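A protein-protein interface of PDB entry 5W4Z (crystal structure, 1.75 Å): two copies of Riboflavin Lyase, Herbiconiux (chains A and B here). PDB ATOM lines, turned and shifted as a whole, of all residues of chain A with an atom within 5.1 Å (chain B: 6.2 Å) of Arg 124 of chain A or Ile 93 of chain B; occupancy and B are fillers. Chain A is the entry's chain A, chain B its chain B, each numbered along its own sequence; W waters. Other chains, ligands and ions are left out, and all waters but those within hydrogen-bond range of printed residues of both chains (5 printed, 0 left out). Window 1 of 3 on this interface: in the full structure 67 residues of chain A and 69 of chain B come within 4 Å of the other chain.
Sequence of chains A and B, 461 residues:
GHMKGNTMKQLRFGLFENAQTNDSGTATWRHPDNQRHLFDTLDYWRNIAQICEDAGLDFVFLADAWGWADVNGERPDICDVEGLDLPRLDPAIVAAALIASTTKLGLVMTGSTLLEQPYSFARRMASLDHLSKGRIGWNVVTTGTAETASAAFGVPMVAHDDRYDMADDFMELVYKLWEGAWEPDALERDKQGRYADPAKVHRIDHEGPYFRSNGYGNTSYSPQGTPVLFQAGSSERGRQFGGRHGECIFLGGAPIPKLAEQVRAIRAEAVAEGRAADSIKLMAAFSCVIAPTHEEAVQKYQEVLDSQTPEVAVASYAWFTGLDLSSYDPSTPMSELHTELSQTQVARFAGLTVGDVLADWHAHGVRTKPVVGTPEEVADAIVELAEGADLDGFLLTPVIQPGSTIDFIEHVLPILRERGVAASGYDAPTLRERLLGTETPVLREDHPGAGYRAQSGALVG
The guanidinium group of Arg 123 of chain A lies within salt-bridge range of the side-chain carboxylate of Asp 90 of chain B (2.8 Å). The backbone NH (N) of Asp 90 of chain B sits at hydrogen-bond distance from the side-chain hydroxyl (OG) of Ser 127 of chain A (2.9 Å). The guanidinium group of Arg 124 of chain B lies close to the guanidinium group of Arg 124 of chain A (3.5 Å).
The side-chain hydroxyl (OG) of Ser 120 of chain B lies within hydrogen-bond range of the guanidinium group (NH1) of Arg 124 of chain B. OD2 of Asp 90 of chain B is in hydrogen-bond range of N of Ile 93 of chain B (3.4 Å). OE1 of Glu 116 of chain B is in salt-bridge range of NH2 of Arg 124 of chain B. The backbone carbonyl oxygen (O) of Arg 123 of chain A sits at hydrogen-bond distance from the side-chain hydroxyl (OG) of Ser 127 of chain A. N of Ala 92 of chain B sits at hydrogen-bond distance from OD2 of Asp 90 of chain B, 3.3 Å away. The side-chain carboxylate (OE1) of Glu 116 of chain A is in salt-bridge range of the guanidinium group (NH2) of Arg 124 of chain A (2.5 Å).
Water W1 bridges OD2 of Asp 90 of chain B and NH1 of Arg 124 of chain A. Water W3 lies within hydrogen-bond range of OD1 of Asp 90 of chain B, O of Ser 120 of chain A, NE of Arg 123 of chain A and N of Arg 124 of chain A. Water W2 lies within hydrogen-bond range of OE2 of Glu 116 of chain A (2.8 Å), NH1 of Arg 124 of chain B (2.9 Å) and OG of Ser 120 of chain B (2.9 Å). Water W4 bridges NE of Arg 124 of chain B (2.9 Å) and NE of Arg 124 of chain A (3.0 Å). Water W5 lies within hydrogen-bond range of the side-chain carboxylate (OE2) of Glu 116 of chain B (3.0 Å), the guanidinium group (NH1) of Arg 124 of chain A (3.1 Å) and the side-chain carboxylate (OD1) of Asp 90 of chain B (3.3 Å).
Among the printed residues, pairs that only touch across the chains: Ile 93 of chain A with Ala 96 of chain B (3.8 Å), Ile 93 of chain A with Arg 124 of chain B (3.7 Å), Ala 96 of chain A with Ile 93 of chain B (3.8 Å), Ala 96 of chain A with Ala 96 of chain B (3.5 Å), Ala 96 of chain A with Ala 97 of chain B (3.6 Å), Ser 120 of chain A with Trp 66 of chain B (3.4 Å), Arg 123 of chain A with Trp 66 of chain B (3.3 Å), Arg 123 of chain A with Pro 91 of chain B (3.4 Å), Arg 124 of chain A with Ile 93 of chain B (3.7 Å), Leu 128 of chain A with Ile 93 of chain B (3.8 Å) and Leu 131 of chain A with Ile 93 of chain B (3.9 Å).
Of the 14 printed residues of chain A, 8 touch a printed residue of chain B. Of the 14 printed residues of chain B, 7 touch a printed residue of chain A. Printed residues of chain B that touch a printed residue of chain A: Trp 66, Asp 90, Pro 91, Ile 93, Ala 96, Ala 97 and Arg 124.
Ile 93 of chain A touches Ala 96 of chain B, and with the chains exchanged Ala 96 of chain A touches Ile 93 of chain B. Ile 93 of chain A touches Arg 124 of chain B, and with the chains exchanged Arg 124 of chain A touches Ile 93 of chain B. Ala 96 of chain A touches its own counterpart, Ala 96 of chain B. Arg 124 of chain A touches its own counterpart, Arg 124 of chain B. Of the 14 pairs that touch across the chains among the printed residues, 6 have their exchanged pair printed and touching as well.
Of chain B, only Ile 93 (3.7 Å) and Arg 124 (3.5 Å) come within 4 Å of Arg 124 of chain A. Ile 93 of chain B touches just these residues of chain A: Ala 96, Arg 124, Leu 128 and Leu 131. Of the printed residues of chain B, Ala 96 of chain A touches Ile 93 (3.8 Å), Ala 96 (3.5 Å) and Ala 97 (3.6 Å). Of the printed residues of chain B, Ser 127 of chain A touches Asp 90. The nearest residue of chain B that does not touch Arg 124 of chain A is Asp 90 of chain B (4.2 Å). The nearest residue of chain A that does not touch Ile 93 of chain B is Ser 127 of chain A (4.1 Å).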
ATOM      1  N   ALA A  92      21.778 -25.544   0.220  1.00  0.00           N
ATOM      2  CA  ALA A  92      21.905 -25.810   1.649  1.00  0.00           C
ATOM      3  C   ALA A  92      21.991 -27.302   1.923  1.00  0.00           C
ATOM      4  O   ALA A  92      22.694 -27.734   2.845  1.00  0.00           O
ATOM      5  CB  ALA A  92      20.721 -25.210   2.418  1.00  0.00           C
ATOM      6  N   ILE A  93      21.238 -28.100   1.168  1.00  0.00           N
ATOM      7  CA  ILE A  93      21.276 -29.546   1.361  1.00  0.00           C
ATOM      8  C   ILE A  93      22.642 -30.091   0.964  1.00  0.00           C
ATOM      9  O   ILE A  93      23.223 -30.928   1.668  1.00  0.00           O
ATOM     10  CB  ILE A  93      20.151 -30.212   0.553  1.00  0.00           C
ATOM     11  CG1 ILE A  93      18.784 -29.708   1.041  1.00  0.00           C
ATOM     12  CG2 ILE A  93      20.267 -31.715   0.641  1.00  0.00           C
ATOM     13  CD1 ILE A  93      18.512 -30.011   2.526  1.00  0.00           C
ATOM     14  N   ALA A  96      25.115 -29.051   3.723  1.00  0.00           N
ATOM     15  CA  ALA A  96      24.982 -29.859   4.931  1.00  0.00           C
ATOM     16  C   ALA A  96      25.598 -31.238   4.741  1.00  0.00           C
ATOM     17  O   ALA A  96      26.240 -31.766   5.653  1.00  0.00           O
ATOM     18  CB  ALA A  96      23.506 -29.984   5.329  1.00  0.00           C
ATOM     19  N   GLU A 116      13.523 -16.316   0.145  1.00  0.00           N
ATOM     20  CA  GLU A 116      13.622 -16.982   1.439  1.00  0.00           C
ATOM     21  C   GLU A 116      12.813 -16.224   2.477  1.00  0.00           C
ATOM     22  O   GLU A 116      12.701 -14.997   2.425  1.00  0.00           O
ATOM     23  CB  GLU A 116      15.078 -17.081   1.911  1.00  0.00           C
ATOM     24  CG  GLU A 116      15.968 -17.999   1.069  1.00  0.00           C
ATOM     25  CD  GLU A 116      15.750 -19.472   1.383  1.00  0.00           C
ATOM     26  OE1 GLU A 116      15.039 -19.770   2.367  1.00  0.00           O
ATOM     27  OE2 GLU A 116      16.295 -20.328   0.651  1.00  0.00           O
ATOM     28  N   SER A 120      12.862 -18.703   8.885  1.00  0.00           N
ATOM     29  CA  SER A 120      13.295 -20.076   8.629  1.00  0.00           C
ATOM     30  C   SER A 120      14.703 -20.115   8.055  1.00  0.00           C
ATOM     31  O   SER A 120      15.465 -21.034   8.365  1.00  0.00           O
ATOM     32  CB  SER A 120      12.313 -20.800   7.696  1.00  0.00           C
ATOM     33  OG  SER A 120      12.018 -20.031   6.539  1.00  0.00           O
ATOM     34  N   PHE A 121      15.076 -19.113   7.259  1.00  0.00           N
ATOM     35  CA  PHE A 121      16.436 -19.053   6.739  1.00  0.00           C
ATOM     36  C   PHE A 121      17.453 -18.888   7.863  1.00  0.00           C
ATOM     37  O   PHE A 121      18.520 -19.526   7.852  1.00  0.00           O
ATOM     38  CB  PHE A 121      16.548 -17.905   5.729  1.00  0.00           C
ATOM     39  CG  PHE A 121      17.903 -17.817   5.086  1.00  0.00           C
ATOM     40  CD1 PHE A 121      18.306 -18.757   4.150  1.00  0.00           C
ATOM     41  CD2 PHE A 121      18.778 -16.787   5.432  1.00  0.00           C
ATOM     42  CE1 PHE A 121      19.583 -18.685   3.564  1.00  0.00           C
ATOM     43  CE2 PHE A 121      20.028 -16.711   4.860  1.00  0.00           C
ATOM     44  CZ  PHE A 121      20.435 -17.654   3.925  1.00  0.00           C
ATOM     45  N   ALA A 122      17.150 -18.027   8.837  1.00  0.00           N
ATOM     46  CA  ALA A 122      18.061 -17.828   9.957  1.00  0.00           C
ATOM     47  C   ALA A 122      18.281 -19.127  10.716  1.00  0.00           C
ATOM     48  O   ALA A 122      19.417 -19.467  11.069  1.00  0.00           O
ATOM     49  CB  ALA A 122      17.514 -16.743  10.899  1.00  0.00           C
ATOM     50  N   ARG A 123      17.195 -19.872  10.979  1.00  0.00           N
ATOM     51  CA  ARG A 123      17.340 -21.158  11.654  1.00  0.00           C
ATOM     52  C   ARG A 123      18.193 -22.118  10.828  1.00  0.00           C
ATOM     53  O   ARG A 123      19.012 -22.859  11.378  1.00  0.00           O
ATOM     54  CB  ARG A 123      15.964 -21.770  11.934  1.00  0.00           C
ATOM     55  CG  ARG A 123      16.050 -23.015  12.807  1.00  0.00           C
ATOM     56  CD  ARG A 123      14.679 -23.623  13.151  1.00  0.00           C
ATOM     57  NE  ARG A 123      14.170 -24.521  12.133  1.00  0.00           N
ATOM     58  CZ  ARG A 123      13.151 -25.346  12.337  1.00  0.00           C
ATOM     59  NH1 ARG A 123      12.504 -25.318  13.512  1.00  0.00           N
ATOM     60  NH2 ARG A 123      12.746 -26.164  11.369  1.00  0.00           N
ATOM     61  N   ARG A 124      17.979 -22.141   9.513  1.00  0.00           N
ATOM     62  CA  ARG A 124      18.708 -23.065   8.647  1.00  0.00           C
ATOM     63  C   ARG A 124      20.197 -22.755   8.655  1.00  0.00           C
ATOM     64  O   ARG A 124      21.029 -23.656   8.804  1.00  0.00           O
ATOM     65  CB  ARG A 124      18.161 -22.984   7.223  1.00  0.00           C
ATOM     66  CG  ARG A 124      18.658 -24.067   6.275  1.00  0.00           C
ATOM     67  CD  ARG A 124      17.551 -24.495   5.317  1.00  0.00           C
ATOM     68  NE  ARG A 124      17.184 -23.412   4.420  1.00  0.00           N
ATOM     69  CZ  ARG A 124      16.000 -22.810   4.383  1.00  0.00           C
ATOM     70  NH1 ARG A 124      15.004 -23.182   5.182  1.00  0.00           N
ATOM     71  NH2 ARG A 124      15.822 -21.822   3.525  1.00  0.00           N
ATOM     72  N   MET A 125      20.554 -21.477   8.491  1.00  0.00           N
ATOM     73  CA  MET A 125      21.967 -21.113   8.451  1.00  0.00           C
ATOM     74  C   MET A 125      22.641 -21.359   9.788  1.00  0.00           C
ATOM     75  O   MET A 125      23.783 -21.838   9.837  1.00  0.00           O
ATOM     76  CB  MET A 125      22.132 -19.639   8.052  1.00  0.00           C
ATOM     77  CG  MET A 125      21.683 -19.317   6.628  1.00  0.00           C
ATOM     78  SD  MET A 125      22.391 -20.419   5.343  1.00  0.00           S
ATOM     79  CE  MET A 125      24.139 -20.171   5.681  1.00  0.00           C
ATOM     80  N   ALA A 126      21.965 -21.020  10.886  1.00  0.00           N
ATOM     81  CA  ALA A 126      22.565 -21.245  12.191  1.00  0.00           C
ATOM     82  C   ALA A 126      22.738 -22.730  12.469  1.00  0.00           C
ATOM     83  O   ALA A 126      23.694 -23.120  13.142  1.00  0.00           O
ATOM     84  CB  ALA A 126      21.730 -20.570  13.288  1.00  0.00           C
ATOM     85  N   SER A 127      21.825 -23.573  11.963  1.00  0.00           N
ATOM     86  CA  SER A 127      21.991 -25.015  12.106  1.00  0.00           C
ATOM     87  C   SER A 127      23.224 -25.504  11.356  1.00  0.00           C
ATOM     88  O   SER A 127      23.991 -26.335  11.865  1.00  0.00           O
ATOM     89  CB  SER A 127      20.735 -25.739  11.606  1.00  0.00           C
ATOM     90  OG  SER A 127      19.588 -25.332  12.379  1.00  0.00           O
ATOM     91  N   LEU A 128      23.431 -25.007  10.137  1.00  0.00           N
ATOM     92  CA  LEU A 128      24.657 -25.344   9.423  1.00  0.00           C
ATOM     93  C   LEU A 128      25.885 -24.880  10.196  1.00  0.00           C
ATOM     94  O   LEU A 128      26.901 -25.578  10.230  1.00  0.00           O
ATOM     95  CB  LEU A 128      24.648 -24.720   8.029  1.00  0.00           C
ATOM     96  CG  LEU A 128      23.695 -25.359   7.021  1.00  0.00           C
ATOM     97  CD1 LEU A 128      23.426 -24.404   5.873  1.00  0.00           C
ATOM     98  CD2 LEU A 128      24.334 -26.655   6.496  1.00  0.00           C
ATOM     99  N   LEU A 131      26.455 -27.244  13.315  1.00  0.00           N
ATOM    100  CA  LEU A 131      26.921 -28.585  12.953  1.00  0.00           C
ATOM    101  C   LEU A 131      28.324 -28.570  12.348  1.00  0.00           C
ATOM    102  O   LEU A 131      29.085 -29.524  12.554  1.00  0.00           O
ATOM    103  CB  LEU A 131      25.946 -29.252  11.973  1.00  0.00           C
ATOM    104  CG  LEU A 131      24.581 -29.587  12.570  1.00  0.00           C
ATOM    105  CD1 LEU A 131      23.694 -30.353  11.571  1.00  0.00           C
ATOM    106  CD2 LEU A 131      24.746 -30.366  13.896  1.00  0.00           C
ATOM    107  N   TRP B  66       8.091 -25.000  15.457  1.00  0.00           N
ATOM    108  CA  TRP B  66       8.536 -23.658  15.100  1.00  0.00           C
ATOM    109  C   TRP B  66       8.317 -22.640  16.201  1.00  0.00           C
ATOM    110  O   TRP B  66       9.056 -21.649  16.265  1.00  0.00           O
ATOM    111  CB  TRP B  66       7.831 -23.170  13.828  1.00  0.00           C
ATOM    112  CG  TRP B  66       8.418 -23.702  12.567  1.00  0.00           C
ATOM    113  CD1 TRP B  66       7.904 -24.687  11.763  1.00  0.00           C
ATOM    114  CD2 TRP B  66       9.648 -23.285  11.952  1.00  0.00           C
ATOM    115  NE1 TRP B  66       8.735 -24.898  10.686  1.00  0.00           N
ATOM    116  CE2 TRP B  66       9.806 -24.045  10.774  1.00  0.00           C
ATOM    117  CE3 TRP B  66      10.622 -22.333  12.281  1.00  0.00           C
ATOM    118  CZ2 TRP B  66      10.900 -23.891   9.927  1.00  0.00           C
ATOM    119  CZ3 TRP B  66      11.711 -22.173  11.428  1.00  0.00           C
ATOM    120  CH2 TRP B  66      11.839 -22.951  10.269  1.00  0.00           C
ATOM    121  N   ASP B  90      17.306 -27.081  12.702  1.00  0.00           N
ATOM    122  CA  ASP B  90      16.430 -27.401  11.579  1.00  0.00           C
ATOM    123  C   ASP B  90      16.574 -28.869  11.176  1.00  0.00           C
ATOM    124  O   ASP B  90      17.693 -29.322  10.887  1.00  0.00           O
ATOM    125  CB  ASP B  90      16.750 -26.512  10.386  1.00  0.00           C
ATOM    126  CG  ASP B  90      15.833 -26.789   9.206  1.00  0.00           C
ATOM    127  OD1 ASP B  90      14.626 -26.478   9.302  1.00  0.00           O
ATOM    128  OD2 ASP B  90      16.313 -27.320   8.191  1.00  0.00           O
ATOM    129  N   PRO B  91      15.473 -29.633  11.124  1.00  0.00           N
ATOM    130  CA  PRO B  91      15.581 -31.072  10.788  1.00  0.00           C
ATOM    131  C   PRO B  91      16.157 -31.373   9.421  1.00  0.00           C
ATOM    132  O   PRO B  91      16.832 -32.404   9.250  1.00  0.00           O
ATOM    133  CB  PRO B  91      14.122 -31.561  10.847  1.00  0.00           C
ATOM    134  CG  PRO B  91      13.339 -30.529  11.552  1.00  0.00           C
ATOM    135  CD  PRO B  91      14.112 -29.222  11.520  1.00  0.00           C
ATOM    136  N   ALA B  92      15.853 -30.549   8.414  1.00  0.00           N
ATOM    137  CA  ALA B  92      16.348 -30.840   7.074  1.00  0.00           C
ATOM    138  C   ALA B  92      17.869 -30.795   7.031  1.00  0.00           C
ATOM    139  O   ALA B  92      18.498 -31.572   6.308  1.00  0.00           O
ATOM    140  CB  ALA B  92      15.784 -29.842   6.067  1.00  0.00           C
ATOM    141  N   ILE B  93      18.465 -29.903   7.819  1.00  0.00           N
ATOM    142  CA  ILE B  93      19.920 -29.791   7.858  1.00  0.00           C
ATOM    143  C   ILE B  93      20.515 -30.993   8.580  1.00  0.00           C
ATOM    144  O   ILE B  93      21.496 -31.592   8.124  1.00  0.00           O
ATOM    145  CB  ILE B  93      20.336 -28.461   8.513  1.00  0.00           C
ATOM    146  CG1 ILE B  93      19.884 -27.261   7.663  1.00  0.00           C
ATOM    147  CG2 ILE B  93      21.856 -28.409   8.764  1.00  0.00           C
ATOM    148  CD1 ILE B  93      20.460 -27.244   6.239  1.00  0.00           C
ATOM    149  N   VAL B  94      19.936 -31.361   9.721  1.00  0.00           N
ATOM    150  CA  VAL B  94      20.350 -32.596  10.397  1.00  0.00           C
ATOM    151  C   VAL B  94      20.226 -33.793   9.465  1.00  0.00           C
ATOM    152  O   VAL B  94      21.148 -34.618   9.359  1.00  0.00           O
ATOM    153  CB  VAL B  94      19.545 -32.805  11.698  1.00  0.00           C
ATOM    154  CG1 VAL B  94      19.955 -34.125  12.377  1.00  0.00           C
ATOM    155  CG2 VAL B  94      19.782 -31.647  12.657  1.00  0.00           C
ATOM    156  N   ALA B  95      19.078 -33.924   8.782  1.00  0.00           N
ATOM    157  CA  ALA B  95      18.879 -35.065   7.889  1.00  0.00           C
ATOM    158  C   ALA B  95      19.932 -35.101   6.789  1.00  0.00           C
ATOM    159  O   ALA B  95      20.443 -36.175   6.448  1.00  0.00           O
ATOM    160  CB  ALA B  95      17.484 -35.019   7.245  1.00  0.00           C
ATOM    161  N   ALA B  96      20.242 -33.936   6.203  1.00  0.00           N
ATOM    162  CA  ALA B  96      21.196 -33.889   5.099  1.00  0.00           C
ATOM    163  C   ALA B  96      22.580 -34.314   5.566  1.00  0.00           C
ATOM    164  O   ALA B  96      23.294 -35.025   4.844  1.00  0.00           O
ATOM    165  CB  ALA B  96      21.245 -32.482   4.490  1.00  0.00           C
ATOM    166  N   ALA B  97      22.980 -33.867   6.761  1.00  0.00           N
ATOM    167  CA  ALA B  97      24.259 -34.284   7.335  1.00  0.00           C
ATOM    168  C   ALA B  97      24.281 -35.787   7.581  1.00  0.00           C
ATOM    169  O   ALA B  97      25.310 -36.445   7.383  1.00  0.00           O
ATOM    170  CB  ALA B  97      24.522 -33.534   8.641  1.00  0.00           C
ATOM    171  N   LEU B  98      23.156 -36.351   8.011  1.00  0.00           N
ATOM    172  CA  LEU B  98      23.128 -37.782   8.277  1.00  0.00           C
ATOM    173  C   LEU B  98      23.131 -38.625   7.006  1.00  0.00           C
ATOM    174  O   LEU B  98      23.481 -39.809   7.078  1.00  0.00           O
ATOM    175  CB  LEU B  98      21.922 -38.142   9.133  1.00  0.00           C
ATOM    176  CG  LEU B  98      22.083 -37.721  10.592  1.00  0.00           C
ATOM    177  CD1 LEU B  98      20.848 -38.104  11.409  1.00  0.00           C
ATOM    178  CD2 LEU B  98      23.351 -38.342  11.168  1.00  0.00           C
ATOM    179  N   MET B 109      11.854 -36.523   8.135  1.00  0.00           N
ATOM    180  CA  MET B 109      11.868 -35.225   8.791  1.00  0.00           C
ATOM    181  C   MET B 109      10.482 -34.610   8.790  1.00  0.00           C
ATOM    182  O   MET B 109       9.763 -34.660   7.788  1.00  0.00           O
ATOM    183  CB  MET B 109      12.831 -34.268   8.116  1.00  0.00           C
ATOM    184  CG  MET B 109      12.694 -34.244   6.619  1.00  0.00           C
ATOM    185  SD  MET B 109      13.458 -32.753   5.950  1.00  0.00           S
ATOM    186  CE  MET B 109      12.161 -31.523   6.250  1.00  0.00           C
ATOM    187  N   GLU B 116       6.276 -23.562   5.462  1.00  0.00           N
ATOM    188  CA  GLU B 116       7.137 -23.751   4.309  1.00  0.00           C
ATOM    189  C   GLU B 116       6.476 -23.181   3.057  1.00  0.00           C
ATOM    190  O   GLU B 116       5.246 -23.154   2.927  1.00  0.00           O
ATOM    191  CB  GLU B 116       7.450 -25.237   4.118  1.00  0.00           C
ATOM    192  CG  GLU B 116       8.175 -25.890   5.298  1.00  0.00           C
ATOM    193  CD  GLU B 116       9.664 -25.603   5.308  1.00  0.00           C
ATOM    194  OE1 GLU B 116      10.133 -24.938   4.362  1.00  0.00           O
ATOM    195  OE2 GLU B 116      10.361 -26.043   6.252  1.00  0.00           O
ATOM    196  N   SER B 120       9.985 -23.972  -2.786  1.00  0.00           N
ATOM    197  CA  SER B 120      11.290 -24.185  -2.172  1.00  0.00           C
ATOM    198  C   SER B 120      11.342 -25.509  -1.419  1.00  0.00           C
ATOM    199  O   SER B 120      12.339 -26.238  -1.500  1.00  0.00           O
ATOM    200  CB  SER B 120      11.617 -23.021  -1.240  1.00  0.00           C
ATOM    201  OG  SER B 120      12.644 -23.381  -0.339  1.00  0.00           O
ATOM    202  N   ARG B 124      13.887 -28.752  -1.890  1.00  0.00           N
ATOM    203  CA  ARG B 124      14.696 -29.197  -0.756  1.00  0.00           C
ATOM    204  C   ARG B 124      14.523 -30.691  -0.507  1.00  0.00           C
ATOM    205  O   ARG B 124      15.508 -31.414  -0.297  1.00  0.00           O
ATOM    206  CB  ARG B 124      14.313 -28.408   0.500  1.00  0.00           C
ATOM    207  CG  ARG B 124      15.193 -28.674   1.716  1.00  0.00           C
ATOM    208  CD  ARG B 124      14.841 -27.751   2.895  1.00  0.00           C
ATOM    209  NE  ARG B 124      14.827 -26.357   2.455  1.00  0.00           N
ATOM    210  CZ  ARG B 124      13.769 -25.557   2.510  1.00  0.00           C
ATOM    211  NH1 ARG B 124      13.868 -24.316   2.054  1.00  0.00           N
ATOM    212  NH2 ARG B 124      12.620 -25.990   3.017  1.00  0.00           N
HETATM  213  O   HOH W   1      15.236 -26.258   5.945  1.00  0.00           O
HETATM  214  O   HOH W   2      15.520 -22.940   0.084  1.00  0.00           O
HETATM  215  O   HOH W   3      14.939 -23.748   9.275  1.00  0.00           O
HETATM  216  O   HOH W   4      17.156 -24.861   1.750  1.00  0.00           O
HETATM  217  O   HOH W   5      13.059 -24.851   6.900  1.00  0.00           O
